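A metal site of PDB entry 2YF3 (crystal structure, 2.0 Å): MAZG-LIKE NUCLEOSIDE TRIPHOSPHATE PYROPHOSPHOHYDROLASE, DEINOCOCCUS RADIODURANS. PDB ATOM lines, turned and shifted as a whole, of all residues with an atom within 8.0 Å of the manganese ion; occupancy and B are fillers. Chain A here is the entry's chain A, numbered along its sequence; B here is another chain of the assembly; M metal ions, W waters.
Of the 16 residues printed, 4 come within 4 Å of the manganese ion.
Along chain A the residues within 4 Å of the manganese ion span positions 53 to 88.
The manganese ion is bound by the side-chain carboxylate of Glu 56, the side-chain carboxylate of Asp 88, the side-chain carboxylate of Glu 85, the side-chain carboxylate of Glu 53, water W1 and water W2.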
ATOM      1  N   LEU A  49      28.689  23.955  14.482  1.00  0.00           N
ATOM      2  CA  LEU A  49      27.662  23.546  13.516  1.00  0.00           C
ATOM      3  C   LEU A  49      27.331  22.029  13.573  1.00  0.00           C
ATOM      4  O   LEU A  49      26.156  21.609  13.465  1.00  0.00           O
ATOM      5  CB  LEU A  49      28.097  23.936  12.092  1.00  0.00           C
ATOM      6  CG  LEU A  49      28.433  25.419  11.969  1.00  0.00           C
ATOM      7  CD1 LEU A  49      29.209  25.651  10.655  1.00  0.00           C
ATOM      8  CD2 LEU A  49      27.123  26.242  11.969  1.00  0.00           C
ATOM      9  N   GLU A  52      25.210  21.371  16.736  1.00  0.00           N
ATOM     10  CA  GLU A  52      23.854  21.843  16.450  1.00  0.00           C
ATOM     11  C   GLU A  52      23.035  20.837  15.614  1.00  0.00           C
ATOM     12  O   GLU A  52      21.934  20.420  16.012  1.00  0.00           O
ATOM     13  CB  GLU A  52      23.854  23.235  15.799  1.00  0.00           C
ATOM     14  CG  GLU A  52      23.911  24.322  16.919  1.00  0.00           C
ATOM     15  CD  GLU A  52      24.419  25.744  16.503  1.00  0.00           C
ATOM     16  OE1 GLU A  52      24.569  26.049  15.294  1.00  0.00           O
ATOM     17  OE2 GLU A  52      24.691  26.542  17.456  1.00  0.00           O
ATOM     18  N   GLU A  53      23.566  20.448  14.474  1.00  0.00           N
ATOM     19  CA  GLU A  53      22.826  19.534  13.595  1.00  0.00           C
ATOM     20  C   GLU A  53      22.709  18.130  14.195  1.00  0.00           C
ATOM     21  O   GLU A  53      21.666  17.498  14.086  1.00  0.00           O
ATOM     22  CB  GLU A  53      23.424  19.497  12.198  1.00  0.00           C
ATOM     23  CG  GLU A  53      23.518  20.893  11.532  1.00  0.00           C
ATOM     24  CD  GLU A  53      22.166  21.598  11.379  1.00  0.00           C
ATOM     25  OE1 GLU A  53      21.100  20.980  11.551  1.00  0.00           O
ATOM     26  OE2 GLU A  53      22.147  22.776  11.087  1.00  0.00           O
ATOM     27  N   SER A  54      23.792  17.634  14.839  1.00  0.00           N
ATOM     28  CA  SER A  54      23.743  16.348  15.533  1.00  0.00           C
ATOM     29  C   SER A  54      22.665  16.366  16.623  1.00  0.00           C
ATOM     30  O   SER A  54      21.963  15.362  16.782  1.00  0.00           O
ATOM     31  CB  SER A  54      25.112  16.001  16.156  1.00  0.00           C
ATOM     32  OG  SER A  54      25.967  15.641  15.072  1.00  0.00           O
ATOM     33  N   ALA A  55      22.565  17.483  17.367  1.00  0.00           N
ATOM     34  CA  ALA A  55      21.497  17.618  18.355  1.00  0.00           C
ATOM     35  C   ALA A  55      20.068  17.569  17.733  1.00  0.00           C
ATOM     36  O   ALA A  55      19.189  16.906  18.292  1.00  0.00           O
ATOM     37  CB  ALA A  55      21.688  18.840  19.309  1.00  0.00           C
ATOM     38  N   GLU A  56      19.876  18.236  16.597  1.00  0.00           N
ATOM     39  CA  GLU A  56      18.586  18.204  15.878  1.00  0.00           C
ATOM     40  C   GLU A  56      18.237  16.800  15.350  1.00  0.00           C
ATOM     41  O   GLU A  56      17.077  16.374  15.440  1.00  0.00           O
ATOM     42  CB  GLU A  56      18.557  19.256  14.761  1.00  0.00           C
ATOM     43  CG  GLU A  56      18.639  20.703  15.396  1.00  0.00           C
ATOM     44  CD  GLU A  56      18.898  21.864  14.421  1.00  0.00           C
ATOM     45  OE1 GLU A  56      18.566  21.822  13.203  1.00  0.00           O
ATOM     46  OE2 GLU A  56      19.461  22.886  14.908  1.00  0.00           O
ATOM     47  N   VAL A  57      19.241  16.103  14.807  1.00  0.00           N
ATOM     48  CA  VAL A  57      19.024  14.727  14.366  1.00  0.00           C
ATOM     49  C   VAL A  57      18.582  13.873  15.547  1.00  0.00           C
ATOM     50  O   VAL A  57      17.594  13.127  15.427  1.00  0.00           O
ATOM     51  CB  VAL A  57      20.253  14.063  13.738  1.00  0.00           C
ATOM     52  CG1 VAL A  57      19.983  12.516  13.474  1.00  0.00           C
ATOM     53  CG2 VAL A  57      20.636  14.767  12.429  1.00  0.00           C
ATOM     54  N   PRO A  81      11.050  15.253   8.862  1.00  0.00           N
ATOM     55  CA  PRO A  81      11.918  16.027   9.752  1.00  0.00           C
ATOM     56  C   PRO A  81      13.293  15.364  10.023  1.00  0.00           C
ATOM     57  O   PRO A  81      14.320  16.045   9.986  1.00  0.00           O
ATOM     58  CB  PRO A  81      11.105  16.141  11.022  1.00  0.00           C
ATOM     59  CG  PRO A  81       9.560  16.055  10.452  1.00  0.00           C
ATOM     60  CD  PRO A  81       9.765  14.912   9.512  1.00  0.00           C
ATOM     61  N   HIS A  84      15.311  15.688   6.839  1.00  0.00           N
ATOM     62  CA  HIS A  84      15.766  17.091   6.747  1.00  0.00           C
ATOM     63  C   HIS A  84      17.045  17.334   7.610  1.00  0.00           C
ATOM     64  O   HIS A  84      18.061  17.863   7.126  1.00  0.00           O
ATOM     65  CB  HIS A  84      14.588  17.996   7.189  1.00  0.00           C
ATOM     66  CG  HIS A  84      14.863  19.470   7.099  1.00  0.00           C
ATOM     67  ND1 HIS A  84      13.886  20.413   7.285  1.00  0.00           N
ATOM     68  CD2 HIS A  84      15.992  20.150   6.760  1.00  0.00           C
ATOM     69  CE1 HIS A  84      14.418  21.623   7.137  1.00  0.00           C
ATOM     70  NE2 HIS A  84      15.695  21.485   6.824  1.00  0.00           N
ATOM     71  N   GLU A  85      17.012  16.858   8.843  1.00  0.00           N
ATOM     72  CA  GLU A  85      18.147  17.048   9.742  1.00  0.00           C
ATOM     73  C   GLU A  85      19.370  16.207   9.381  1.00  0.00           C
ATOM     74  O   GLU A  85      20.512  16.668   9.567  1.00  0.00           O
ATOM     75  CB  GLU A  85      17.696  16.757  11.182  1.00  0.00           C
ATOM     76  CG  GLU A  85      16.535  17.698  11.666  1.00  0.00           C
ATOM     77  CD  GLU A  85      16.857  19.173  11.449  1.00  0.00           C
ATOM     78  OE1 GLU A  85      18.039  19.520  11.338  1.00  0.00           O
ATOM     79  OE2 GLU A  85      15.916  19.985  11.410  1.00  0.00           O
ATOM     80  N   LEU A  86      19.143  14.986   8.853  1.00  0.00           N
ATOM     81  CA  LEU A  86      20.247  14.170   8.402  1.00  0.00           C
ATOM     82  C   LEU A  86      20.951  14.876   7.224  1.00  0.00           C
ATOM     83  O   LEU A  86      22.179  14.897   7.138  1.00  0.00           O
ATOM     84  CB  LEU A  86      19.775  12.753   8.007  1.00  0.00           C
ATOM     85  CG  LEU A  86      19.398  11.860   9.194  1.00  0.00           C
ATOM     86  CD1 LEU A  86      18.633  10.561   8.727  1.00  0.00           C
ATOM     87  CD2 LEU A  86      20.680  11.518   9.974  1.00  0.00           C
ATOM     88  N   ALA A  87      20.150  15.443   6.312  1.00  0.00           N
ATOM     89  CA  ALA A  87      20.704  16.293   5.233  1.00  0.00           C
ATOM     90  C   ALA A  87      21.420  17.545   5.744  1.00  0.00           C
ATOM     91  O   ALA A  87      22.488  17.896   5.204  1.00  0.00           O
ATOM     92  CB  ALA A  87      19.567  16.666   4.239  1.00  0.00           C
ATOM     93  N   ASP A  88      20.838  18.241   6.740  1.00  0.00           N
ATOM     94  CA  ASP A  88      21.540  19.376   7.367  1.00  0.00           C
ATOM     95  C   ASP A  88      22.881  18.867   7.915  1.00  0.00           C
ATOM     96  O   ASP A  88      23.872  19.570   7.836  1.00  0.00           O
ATOM     97  CB  ASP A  88      20.780  19.992   8.545  1.00  0.00           C
ATOM     98  CG  ASP A  88      19.675  20.946   8.126  1.00  0.00           C
ATOM     99  OD1 ASP A  88      19.554  21.213   6.891  1.00  0.00           O
ATOM    100  OD2 ASP A  88      18.936  21.407   9.045  1.00  0.00           O
ATOM    101  N   LEU A  89      22.916  17.659   8.487  1.00  0.00           N
ATOM    102  CA  LEU A  89      24.173  17.138   9.068  1.00  0.00           C
ATOM    103  C   LEU A  89      25.210  16.878   7.945  1.00  0.00           C
ATOM    104  O   LEU A  89      26.387  17.230   8.084  1.00  0.00           O
ATOM    105  CB  LEU A  89      23.948  15.874   9.928  1.00  0.00           C
ATOM    106  CG  LEU A  89      25.209  15.289  10.608  1.00  0.00           C
ATOM    107  CD1 LEU A  89      25.992  16.324  11.513  1.00  0.00           C
ATOM    108  CD2 LEU A  89      24.805  14.052  11.419  1.00  0.00           C
ATOM    109  N   VAL A  92      26.738  20.282   6.868  1.00  0.00           N
ATOM    110  CA  VAL A  92      27.810  20.914   7.698  1.00  0.00           C
ATOM    111  C   VAL A  92      29.050  20.017   7.847  1.00  0.00           C
ATOM    112  O   VAL A  92      30.124  20.501   8.257  1.00  0.00           O
ATOM    113  CB  VAL A  92      27.293  21.362   9.095  1.00  0.00           C
ATOM    114  CG1 VAL A  92      26.097  22.348   8.945  1.00  0.00           C
ATOM    115  CG2 VAL A  92      26.825  20.122   9.871  1.00  0.00           C
ATOM    116  N   VAL B 111      17.755  20.906   0.175  1.00  0.00           N
ATOM    117  CA  VAL B 111      18.418  21.655   1.231  1.00  0.00           C
ATOM    118  C   VAL B 111      19.458  22.617   0.624  1.00  0.00           C
ATOM    119  O   VAL B 111      19.483  23.803   0.976  1.00  0.00           O
ATOM    120  CB  VAL B 111      18.988  20.671   2.289  1.00  0.00           C
ATOM    121  CG1 VAL B 111      20.014  21.357   3.282  1.00  0.00           C
ATOM    122  CG2 VAL B 111      17.795  19.968   3.060  1.00  0.00           C
HETATM  123 MN    MN M   1      18.941  21.542  11.152  1.00  0.00          MN
HETATM  124  O   HOH W   1      19.709  23.754  11.106  1.00  0.00           O
HETATM  125  O   HOH W   2      16.781  22.459  10.756  1.00  0.00           O
